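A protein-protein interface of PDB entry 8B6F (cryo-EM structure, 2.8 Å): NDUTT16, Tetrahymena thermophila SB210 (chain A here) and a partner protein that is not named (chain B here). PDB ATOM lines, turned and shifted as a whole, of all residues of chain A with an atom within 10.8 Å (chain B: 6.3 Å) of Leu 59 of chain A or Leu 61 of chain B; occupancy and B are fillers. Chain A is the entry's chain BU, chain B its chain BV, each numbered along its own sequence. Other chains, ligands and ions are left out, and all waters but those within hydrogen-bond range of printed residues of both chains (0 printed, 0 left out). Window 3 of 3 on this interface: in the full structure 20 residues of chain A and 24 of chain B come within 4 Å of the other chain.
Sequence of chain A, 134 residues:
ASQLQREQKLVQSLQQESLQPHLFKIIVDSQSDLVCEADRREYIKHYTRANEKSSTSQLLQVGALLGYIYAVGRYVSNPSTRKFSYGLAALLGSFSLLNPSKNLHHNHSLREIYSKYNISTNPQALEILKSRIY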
ATOM      1  N   LYS A  53      -0.819   3.240   9.090  1.00  0.00           N
ATOM      2  CA  LYS A  53      -0.949   2.100   8.192  1.00  0.00           C
ATOM      3  C   LYS A  53      -0.784   2.594   6.761  1.00  0.00           C
ATOM      4  O   LYS A  53      -1.500   3.501   6.327  1.00  0.00           O
ATOM      5  CB  LYS A  53      -2.302   1.410   8.366  1.00  0.00           C
ATOM      6  CG  LYS A  53      -2.502   0.772   9.731  1.00  0.00           C
ATOM      7  CD  LYS A  53      -3.848   0.072   9.819  1.00  0.00           C
ATOM      8  CE  LYS A  53      -4.049  -0.582  11.175  1.00  0.00           C
ATOM      9  NZ  LYS A  53      -3.024  -1.627  11.452  1.00  0.00           N
ATOM     10  N   SER A  54       0.155   1.997   6.035  1.00  0.00           N
ATOM     11  CA  SER A  54       0.464   2.394   4.672  1.00  0.00           C
ATOM     12  C   SER A  54      -0.039   1.344   3.691  1.00  0.00           C
ATOM     13  O   SER A  54      -0.026   0.144   3.977  1.00  0.00           O
ATOM     14  CB  SER A  54       1.971   2.589   4.483  1.00  0.00           C
ATOM     15  OG  SER A  54       2.472   3.582   5.361  1.00  0.00           O
ATOM     16  N   SER A  55      -0.485   1.812   2.525  1.00  0.00           N
ATOM     17  CA  SER A  55      -0.918   0.907   1.472  1.00  0.00           C
ATOM     18  C   SER A  55       0.241   0.160   0.830  1.00  0.00           C
ATOM     19  O   SER A  55       0.004  -0.728   0.005  1.00  0.00           O
ATOM     20  CB  SER A  55      -1.679   1.686   0.398  1.00  0.00           C
ATOM     21  OG  SER A  55      -2.755   2.412   0.965  1.00  0.00           O
ATOM     22  N   THR A  56       1.483   0.499   1.183  1.00  0.00           N
ATOM     23  CA  THR A  56       2.633  -0.139   0.554  1.00  0.00           C
ATOM     24  C   THR A  56       2.658  -1.637   0.829  1.00  0.00           C
ATOM     25  O   THR A  56       3.063  -2.425  -0.032  1.00  0.00           O
ATOM     26  CB  THR A  56       3.926   0.514   1.041  1.00  0.00           C
ATOM     27  OG1 THR A  56       4.038   0.366   2.463  1.00  0.00           O
ATOM     28  CG2 THR A  56       3.942   1.995   0.687  1.00  0.00           C
ATOM     29  N   SER A  57       2.229  -2.053   2.022  1.00  0.00           N
ATOM     30  CA  SER A  57       2.217  -3.478   2.339  1.00  0.00           C
ATOM     31  C   SER A  57       1.264  -4.226   1.417  1.00  0.00           C
ATOM     32  O   SER A  57       1.610  -5.274   0.861  1.00  0.00           O
ATOM     33  CB  SER A  57       1.831  -3.691   3.802  1.00  0.00           C
ATOM     34  OG  SER A  57       0.540  -3.175   4.069  1.00  0.00           O
ATOM     35  N   GLN A  58       0.048  -3.705   1.250  1.00  0.00           N
ATOM     36  CA  GLN A  58      -0.902  -4.341   0.343  1.00  0.00           C
ATOM     37  C   GLN A  58      -0.380  -4.312  -1.085  1.00  0.00           C
ATOM     38  O   GLN A  58      -0.511  -5.293  -1.825  1.00  0.00           O
ATOM     39  CB  GLN A  58      -2.261  -3.643   0.421  1.00  0.00           C
ATOM     40  CG  GLN A  58      -2.745  -3.336   1.830  1.00  0.00           C
ATOM     41  CD  GLN A  58      -2.988  -4.582   2.650  1.00  0.00           C
ATOM     42  OE1 GLN A  58      -4.132  -4.958   2.890  1.00  0.00           O
ATOM     43  NE2 GLN A  58      -1.913  -5.228   3.091  1.00  0.00           N
ATOM     44  N   LEU A  59       0.218  -3.188  -1.485  1.00  0.00           N
ATOM     45  CA  LEU A  59       0.732  -3.053  -2.843  1.00  0.00           C
ATOM     46  C   LEU A  59       1.833  -4.069  -3.120  1.00  0.00           C
ATOM     47  O   LEU A  59       1.879  -4.663  -4.204  1.00  0.00           O
ATOM     48  CB  LEU A  59       1.239  -1.629  -3.067  1.00  0.00           C
ATOM     49  CG  LEU A  59       1.711  -1.290  -4.483  1.00  0.00           C
ATOM     50  CD1 LEU A  59       0.586  -1.458  -5.495  1.00  0.00           C
ATOM     51  CD2 LEU A  59       2.263   0.123  -4.531  1.00  0.00           C
ATOM     52  N   LEU A  60       2.742  -4.272  -2.166  1.00  0.00           N
ATOM     53  CA  LEU A  60       3.818  -5.231  -2.386  1.00  0.00           C
ATOM     54  C   LEU A  60       3.312  -6.665  -2.326  1.00  0.00           C
ATOM     55  O   LEU A  60       3.837  -7.533  -3.033  1.00  0.00           O
ATOM     56  CB  LEU A  60       4.950  -5.006  -1.375  1.00  0.00           C
ATOM     57  CG  LEU A  60       4.770  -5.309   0.120  1.00  0.00           C
ATOM     58  CD1 LEU A  60       4.827  -6.805   0.454  1.00  0.00           C
ATOM     59  CD2 LEU A  60       5.805  -4.553   0.936  1.00  0.00           C
ATOM     60  N   GLN A  61       2.301  -6.942  -1.501  1.00  0.00           N
ATOM     61  CA  GLN A  61       1.701  -8.273  -1.507  1.00  0.00           C
ATOM     62  C   GLN A  61       1.099  -8.586  -2.869  1.00  0.00           C
ATOM     63  O   GLN A  61       1.347  -9.653  -3.442  1.00  0.00           O
ATOM     64  CB  GLN A  61       0.638  -8.380  -0.414  1.00  0.00           C
ATOM     65  CG  GLN A  61       1.203  -8.470   0.992  1.00  0.00           C
ATOM     66  CD  GLN A  61       0.120  -8.494   2.053  1.00  0.00           C
ATOM     67  OE1 GLN A  61      -0.744  -7.619   2.092  1.00  0.00           O
ATOM     68  NE2 GLN A  61       0.160  -9.499   2.917  1.00  0.00           N
ATOM     69  N   VAL A  62       0.300  -7.666  -3.408  1.00  0.00           N
ATOM     70  CA  VAL A  62      -0.310  -7.904  -4.711  1.00  0.00           C
ATOM     71  C   VAL A  62       0.763  -7.976  -5.789  1.00  0.00           C
ATOM     72  O   VAL A  62       0.670  -8.776  -6.725  1.00  0.00           O
ATOM     73  CB  VAL A  62      -1.364  -6.826  -5.024  1.00  0.00           C
ATOM     74  CG1 VAL A  62      -0.746  -5.445  -5.050  1.00  0.00           C
ATOM     75  CG2 VAL A  62      -2.029  -7.120  -6.344  1.00  0.00           C
ATOM     76  N   GLY A  63       1.800  -7.145  -5.673  1.00  0.00           N
ATOM     77  CA  GLY A  63       2.888  -7.207  -6.632  1.00  0.00           C
ATOM     78  C   GLY A  63       3.596  -8.546  -6.619  1.00  0.00           C
ATOM     79  O   GLY A  63       3.917  -9.101  -7.673  1.00  0.00           O
ATOM     80  N   ALA A  64       3.852  -9.085  -5.426  1.00  0.00           N
ATOM     81  CA  ALA A  64       4.484 -10.396  -5.336  1.00  0.00           C
ATOM     82  C   ALA A  64       3.600 -11.474  -5.946  1.00  0.00           C
ATOM     83  O   ALA A  64       4.084 -12.348  -6.674  1.00  0.00           O
ATOM     84  CB  ALA A  64       4.802 -10.724  -3.877  1.00  0.00           C
ATOM     85  N   LEU A  65       2.299 -11.432  -5.658  1.00  0.00           N
ATOM     86  CA  LEU A  65       1.385 -12.418  -6.223  1.00  0.00           C
ATOM     87  C   LEU A  65       1.394 -12.356  -7.744  1.00  0.00           C
ATOM     88  O   LEU A  65       1.554 -13.377  -8.421  1.00  0.00           O
ATOM     89  CB  LEU A  65      -0.024 -12.175  -5.683  1.00  0.00           C
ATOM     90  CG  LEU A  65      -1.105 -13.171  -6.097  1.00  0.00           C
ATOM     91  CD1 LEU A  65      -0.823 -14.521  -5.476  1.00  0.00           C
ATOM     92  CD2 LEU A  65      -2.484 -12.676  -5.708  1.00  0.00           C
ATOM     93  N   LEU A  66       1.219 -11.156  -8.300  1.00  0.00           N
ATOM     94  CA  LEU A  66       1.166 -11.006  -9.749  1.00  0.00           C
ATOM     95  C   LEU A  66       2.493 -11.385 -10.391  1.00  0.00           C
ATOM     96  O   LEU A  66       2.520 -12.017 -11.454  1.00  0.00           O
ATOM     97  CB  LEU A  66       0.783  -9.572 -10.110  1.00  0.00           C
ATOM     98  CG  LEU A  66      -0.601  -9.135  -9.628  1.00  0.00           C
ATOM     99  CD1 LEU A  66      -0.805  -7.651  -9.871  1.00  0.00           C
ATOM    100  CD2 LEU A  66      -1.691  -9.949 -10.309  1.00  0.00           C
ATOM    101  N   GLY A  67       3.603 -11.002  -9.762  1.00  0.00           N
ATOM    102  CA  GLY A  67       4.903 -11.368 -10.297  1.00  0.00           C
ATOM    103  C   GLY A  67       5.128 -12.866 -10.301  1.00  0.00           C
ATOM    104  O   GLY A  67       5.671 -13.418 -11.262  1.00  0.00           O
ATOM    105  N   TYR A  68       4.713 -13.547  -9.232  1.00  0.00           N
ATOM    106  CA  TYR A  68       4.822 -15.001  -9.206  1.00  0.00           C
ATOM    107  C   TYR A  68       4.032 -15.628 -10.347  1.00  0.00           C
ATOM    108  O   TYR A  68       4.543 -16.490 -11.070  1.00  0.00           O
ATOM    109  CB  TYR A  68       4.335 -15.534  -7.858  1.00  0.00           C
ATOM    110  CG  TYR A  68       3.973 -16.999  -7.886  1.00  0.00           C
ATOM    111  CD1 TYR A  68       4.952 -17.980  -7.786  1.00  0.00           C
ATOM    112  CD2 TYR A  68       2.651 -17.403  -8.007  1.00  0.00           C
ATOM    113  CE1 TYR A  68       4.624 -19.321  -7.812  1.00  0.00           C
ATOM    114  CE2 TYR A  68       2.312 -18.740  -8.033  1.00  0.00           C
ATOM    115  CZ  TYR A  68       3.303 -19.694  -7.934  1.00  0.00           C
ATOM    116  OH  TYR A  68       2.968 -21.026  -7.960  1.00  0.00           O
ATOM    117  N   PHE A  95       1.438 -14.998   2.901  1.00  0.00           N
ATOM    118  CA  PHE A  95       1.037 -13.608   3.090  1.00  0.00           C
ATOM    119  C   PHE A  95       0.306 -13.417   4.411  1.00  0.00           C
ATOM    120  O   PHE A  95       0.434 -12.365   5.044  1.00  0.00           O
ATOM    121  CB  PHE A  95       0.149 -13.146   1.930  1.00  0.00           C
ATOM    122  CG  PHE A  95       0.884 -12.938   0.628  1.00  0.00           C
ATOM    123  CD1 PHE A  95       2.236 -12.625   0.603  1.00  0.00           C
ATOM    124  CD2 PHE A  95       0.206 -13.041  -0.576  1.00  0.00           C
ATOM    125  CE1 PHE A  95       2.894 -12.429  -0.595  1.00  0.00           C
ATOM    126  CE2 PHE A  95       0.860 -12.847  -1.777  1.00  0.00           C
ATOM    127  CZ  PHE A  95       2.206 -12.541  -1.786  1.00  0.00           C
ATOM    128  N   GLN B  53       1.285   8.575  -1.139  1.00  0.00           N
ATOM    129  CA  GLN B  53       1.491   7.152  -1.386  1.00  0.00           C
ATOM    130  C   GLN B  53       0.211   6.492  -1.880  1.00  0.00           C
ATOM    131  O   GLN B  53       0.242   5.686  -2.817  1.00  0.00           O
ATOM    132  CB  GLN B  53       1.992   6.461  -0.118  1.00  0.00           C
ATOM    133  CG  GLN B  53       3.413   6.829   0.266  1.00  0.00           C
ATOM    134  CD  GLN B  53       3.901   6.060   1.476  1.00  0.00           C
ATOM    135  OE1 GLN B  53       3.212   5.180   1.986  1.00  0.00           O
ATOM    136  NE2 GLN B  53       5.101   6.391   1.942  1.00  0.00           N
ATOM    137  N   PHE B  56      -0.418   7.486  -5.536  1.00  0.00           N
ATOM    138  CA  PHE B  56       0.476   6.801  -6.461  1.00  0.00           C
ATOM    139  C   PHE B  56       0.069   5.345  -6.625  1.00  0.00           C
ATOM    140  O   PHE B  56       0.043   4.822  -7.744  1.00  0.00           O
ATOM    141  CB  PHE B  56       1.920   6.916  -5.975  1.00  0.00           C
ATOM    142  CG  PHE B  56       2.541   8.261  -6.230  1.00  0.00           C
ATOM    143  CD1 PHE B  56       2.421   8.870  -7.467  1.00  0.00           C
ATOM    144  CD2 PHE B  56       3.235   8.920  -5.230  1.00  0.00           C
ATOM    145  CE1 PHE B  56       2.984  10.104  -7.707  1.00  0.00           C
ATOM    146  CE2 PHE B  56       3.801  10.157  -5.464  1.00  0.00           C
ATOM    147  CZ  PHE B  56       3.674  10.749  -6.704  1.00  0.00           C
ATOM    148  N   ALA B  57      -0.238   4.667  -5.519  1.00  0.00           N
ATOM    149  CA  ALA B  57      -0.665   3.277  -5.616  1.00  0.00           C
ATOM    150  C   ALA B  57      -1.941   3.160  -6.440  1.00  0.00           C
ATOM    151  O   ALA B  57      -2.050   2.298  -7.319  1.00  0.00           O
ATOM    152  CB  ALA B  57      -0.870   2.694  -4.217  1.00  0.00           C
ATOM    153  N   VAL B  58      -2.923   4.021  -6.164  1.00  0.00           N
ATOM    154  CA  VAL B  58      -4.207   3.935  -6.857  1.00  0.00           C
ATOM    155  C   VAL B  58      -4.025   4.187  -8.347  1.00  0.00           C
ATOM    156  O   VAL B  58      -4.547   3.449  -9.190  1.00  0.00           O
ATOM    157  CB  VAL B  58      -5.217   4.919  -6.237  1.00  0.00           C
ATOM    158  CG1 VAL B  58      -6.438   5.093  -7.137  1.00  0.00           C
ATOM    159  CG2 VAL B  58      -5.643   4.442  -4.861  1.00  0.00           C
ATOM    160  N   ALA B  59      -3.284   5.240  -8.694  1.00  0.00           N
ATOM    161  CA  ALA B  59      -3.112   5.582 -10.100  1.00  0.00           C
ATOM    162  C   ALA B  59      -2.323   4.512 -10.840  1.00  0.00           C
ATOM    163  O   ALA B  59      -2.677   4.140 -11.965  1.00  0.00           O
ATOM    164  CB  ALA B  59      -2.430   6.941 -10.226  1.00  0.00           C
ATOM    165  N   GLY B  60      -1.249   4.008 -10.232  1.00  0.00           N
ATOM    166  CA  GLY B  60      -0.489   2.949 -10.872  1.00  0.00           C
ATOM    167  C   GLY B  60      -1.308   1.689 -11.069  1.00  0.00           C
ATOM    168  O   GLY B  60      -1.257   1.064 -12.130  1.00  0.00           O
ATOM    169  N   LEU B  61      -2.077   1.300 -10.050  1.00  0.00           N
ATOM    170  CA  LEU B  61      -2.916   0.114 -10.170  1.00  0.00           C
ATOM    171  C   LEU B  61      -3.974   0.293 -11.251  1.00  0.00           C
ATOM    172  O   LEU B  61      -4.213  -0.617 -12.053  1.00  0.00           O
ATOM    173  CB  LEU B  61      -3.569  -0.200  -8.825  1.00  0.00           C
ATOM    174  CG  LEU B  61      -2.615  -0.681  -7.732  1.00  0.00           C
ATOM    175  CD1 LEU B  61      -3.287  -0.622  -6.375  1.00  0.00           C
ATOM    176  CD2 LEU B  61      -2.135  -2.093  -8.028  1.00  0.00           C
ATOM    177  N   LEU B  62      -4.612   1.464 -11.297  1.00  0.00           N
ATOM    178  CA  LEU B  62      -5.612   1.706 -12.331  1.00  0.00           C
ATOM    179  C   LEU B  62      -4.992   1.630 -13.717  1.00  0.00           C
ATOM    180  O   LEU B  62      -5.564   1.021 -14.629  1.00  0.00           O
ATOM    181  CB  LEU B  62      -6.275   3.067 -12.115  1.00  0.00           C
ATOM    182  CG  LEU B  62      -7.271   3.181 -10.957  1.00  0.00           C
ATOM    183  CD1 LEU B  62      -7.785   4.603 -10.849  1.00  0.00           C
ATOM    184  CD2 LEU B  62      -8.433   2.212 -11.124  1.00  0.00           C
ATOM    185  N   SER B  63      -3.827   2.250 -13.901  1.00  0.00           N
ATOM    186  CA  SER B  63      -3.175   2.220 -15.205  1.00  0.00           C
ATOM    187  C   SER B  63      -2.813   0.795 -15.598  1.00  0.00           C
ATOM    188  O   SER B  63      -3.058   0.369 -16.733  1.00  0.00           O
ATOM    189  CB  SER B  63      -1.937   3.112 -15.179  1.00  0.00           C
ATOM    190  OG  SER B  63      -2.303   4.441 -14.849  1.00  0.00           O
ATOM    191  N   VAL B  64      -2.216   0.041 -14.673  1.00  0.00           N
ATOM    192  CA  VAL B  64      -1.817  -1.329 -14.980  1.00  0.00           C
ATOM    193  C   VAL B  64      -3.038  -2.159 -15.345  1.00  0.00           C
ATOM    194  O   VAL B  64      -3.047  -2.883 -16.348  1.00  0.00           O
ATOM    195  CB  VAL B  64      -1.050  -1.944 -13.795  1.00  0.00           C
ATOM    196  CG1 VAL B  64      -0.848  -3.443 -13.994  1.00  0.00           C
ATOM    197  CG2 VAL B  64       0.291  -1.262 -13.623  1.00  0.00           C
ATOM    198  N   GLY B  65      -4.096  -2.060 -14.537  1.00  0.00           N
ATOM    199  CA  GLY B  65      -5.287  -2.848 -14.801  1.00  0.00           C
ATOM    200  C   GLY B  65      -5.930  -2.496 -16.126  1.00  0.00           C
ATOM    201  O   GLY B  65      -6.299  -3.376 -16.907  1.00  0.00           O
ATOM    202  N   SER B  66      -6.079  -1.199 -16.398  1.00  0.00           N
ATOM    203  CA  SER B  66      -6.703  -0.784 -17.649  1.00  0.00           C
ATOM    204  C   SER B  66      -5.907  -1.278 -18.847  1.00  0.00           C
ATOM    205  O   SER B  66      -6.460  -1.896 -19.764  1.00  0.00           O
ATOM    206  CB  SER B  66      -6.832   0.739 -17.684  1.00  0.00           C
ATOM    207  OG  SER B  66      -7.573   1.211 -16.573  1.00  0.00           O
ATOM    208  N   ALA B 100      -6.030  -7.713 -14.335  1.00  0.00           N
ATOM    209  CA  ALA B 100      -6.838  -6.501 -14.413  1.00  0.00           C
ATOM    210  C   ALA B 100      -7.775  -6.382 -13.218  1.00  0.00           C
ATOM    211  O   ALA B 100      -7.897  -5.310 -12.613  1.00  0.00           O
ATOM    212  CB  ALA B 100      -7.629  -6.487 -15.721  1.00  0.00           C
ATOM    213  N   VAL B 102      -7.475  -7.708 -10.208  1.00  0.00           N
ATOM    214  CA  VAL B 102      -6.747  -7.469  -8.968  1.00  0.00           C
ATOM    215  C   VAL B 102      -6.282  -6.021  -8.895  1.00  0.00           C
ATOM    216  O   VAL B 102      -6.375  -5.379  -7.842  1.00  0.00           O
ATOM    217  CB  VAL B 102      -5.573  -8.459  -8.848  1.00  0.00           C
ATOM    218  CG1 VAL B 102      -4.635  -8.051  -7.740  1.00  0.00           C
ATOM    219  CG2 VAL B 102      -6.091  -9.866  -8.596  1.00  0.00           C
ATOM    220  N   ALA B 103      -5.765  -5.487 -10.003  1.00  0.00           N
ATOM    221  CA  ALA B 103      -5.302  -4.104  -9.995  1.00  0.00           C
ATOM    222  C   ALA B 103      -6.455  -3.145  -9.724  1.00  0.00           C
ATOM    223  O   ALA B 103      -6.363  -2.275  -8.851  1.00  0.00           O
ATOM    224  CB  ALA B 103      -4.626  -3.775 -11.325  1.00  0.00           C
ATOM    225  N   ASN B 104      -7.553  -3.287 -10.469  1.00  0.00           N
ATOM    226  CA  ASN B 104      -8.690  -2.392 -10.283  1.00  0.00           C
ATOM    227  C   ASN B 104      -9.264  -2.521  -8.880  1.00  0.00           C
ATOM    228  O   ASN B 104      -9.606  -1.519  -8.243  1.00  0.00           O
ATOM    229  CB  ASN B 104      -9.770  -2.683 -11.324  1.00  0.00           C
ATOM    230  CG  ASN B 104      -9.293  -2.445 -12.740  1.00  0.00           C
ATOM    231  OD1 ASN B 104      -8.501  -1.542 -12.998  1.00  0.00           O
ATOM    232  ND2 ASN B 104      -9.779  -3.256 -13.670  1.00  0.00           N
ATOM    233  N   ALA B 106      -7.740  -3.549  -6.103  1.00  0.00           N
ATOM    234  CA  ALA B 106      -6.833  -2.962  -5.123  1.00  0.00           C
ATOM    235  C   ALA B 106      -6.944  -1.444  -5.114  1.00  0.00           C
ATOM    236  O   ALA B 106      -6.928  -0.820  -4.048  1.00  0.00           O
ATOM    237  CB  ALA B 106      -5.398  -3.400  -5.408  1.00  0.00           C
ATOM    238  N   ALA B 107      -7.047  -0.830  -6.293  1.00  0.00           N
ATOM    239  CA  ALA B 107      -7.221   0.618  -6.356  1.00  0.00           C
ATOM    240  C   ALA B 107      -8.504   1.043  -5.652  1.00  0.00           C
ATOM    241  O   ALA B 107      -8.509   1.997  -4.867  1.00  0.00           O
ATOM    242  CB  ALA B 107      -7.227   1.079  -7.814  1.00  0.00           C
ATOM    243  N   ILE B 110      -8.158   0.676  -1.851  1.00  0.00           N
ATOM    244  CA  ILE B 110      -7.359   1.751  -1.273  1.00  0.00           C
ATOM    245  C   ILE B 110      -8.170   3.037  -1.215  1.00  0.00           C
ATOM    246  O   ILE B 110      -8.044   3.827  -0.272  1.00  0.00           O
ATOM    247  CB  ILE B 110      -6.052   1.926  -2.070  1.00  0.00           C
ATOM    248  CG1 ILE B 110      -5.154   0.702  -1.867  1.00  0.00           C
ATOM    249  CG2 ILE B 110      -5.327   3.202  -1.654  1.00  0.00           C
ATOM    250  CD1 ILE B 110      -3.921   0.681  -2.739  1.00  0.00           C
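O of Ser 54 of chain A is in hydrogen-bond range of OG of Ser 57 of chain A, 3.4 Å away.
Hydrophobic or aromatic side chains of chain B that line the printed part of chain A: Leu 61, Val 102 and Ile 110. Along chain B the printed residues that touch a printed residue of chain A span positions 53 to 110. Of the 17 printed residues of chain A, 5 touch a printed residue of chain B. Hydrophobic or aromatic side chains of chain A within 4 Å of the printed part of chain B: Leu 59 and Val 62.
Among the printed residues, merely in contact across the chains: Ser 54 of chain A with Gln 53 of chain B, Ser 55 of chain A with Ile 110 of chain B, Thr 56 of chain A with Gln 53 of chain B, Leu 59 of chain A with Leu 61 of chain B and Val 62 of chain A with Val 102 of chain B.
Of chain B, only Leu 61 (3.8 Å) comes within 4 Å of Leu 59 of chain A. No residue of chain A comes within 4 Å of Ala 57 of chain B. No residue of chain A comes within 4 Å of Val 58 of chain B. No residue of chain A comes within 4 Å of Gly 60 of chain B. No residue of chain A comes within 4 Å of Val 64 of chain B. No residue of chain A comes within 4 Å of Gly 65 of chain B. No residue of chain A comes within 4 Å of Ala 103 of chain B. No residue of chain A comes within 4 Å of Ala 106 of chain B. Printed residues of chain B within 4 Å of Val 62 of chain A: Val 102. Of the printed residues of chain B, Ser 54 of chain A touches Gln 53. Of the printed residues of chain A, Val 102 of chain B touches Val 62. Of the printed residues of chain B, Ser 55 of chain A touches Ile 110 (3.8 Å). Gln 58 of chain A touches none of the printed residues of chain B.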
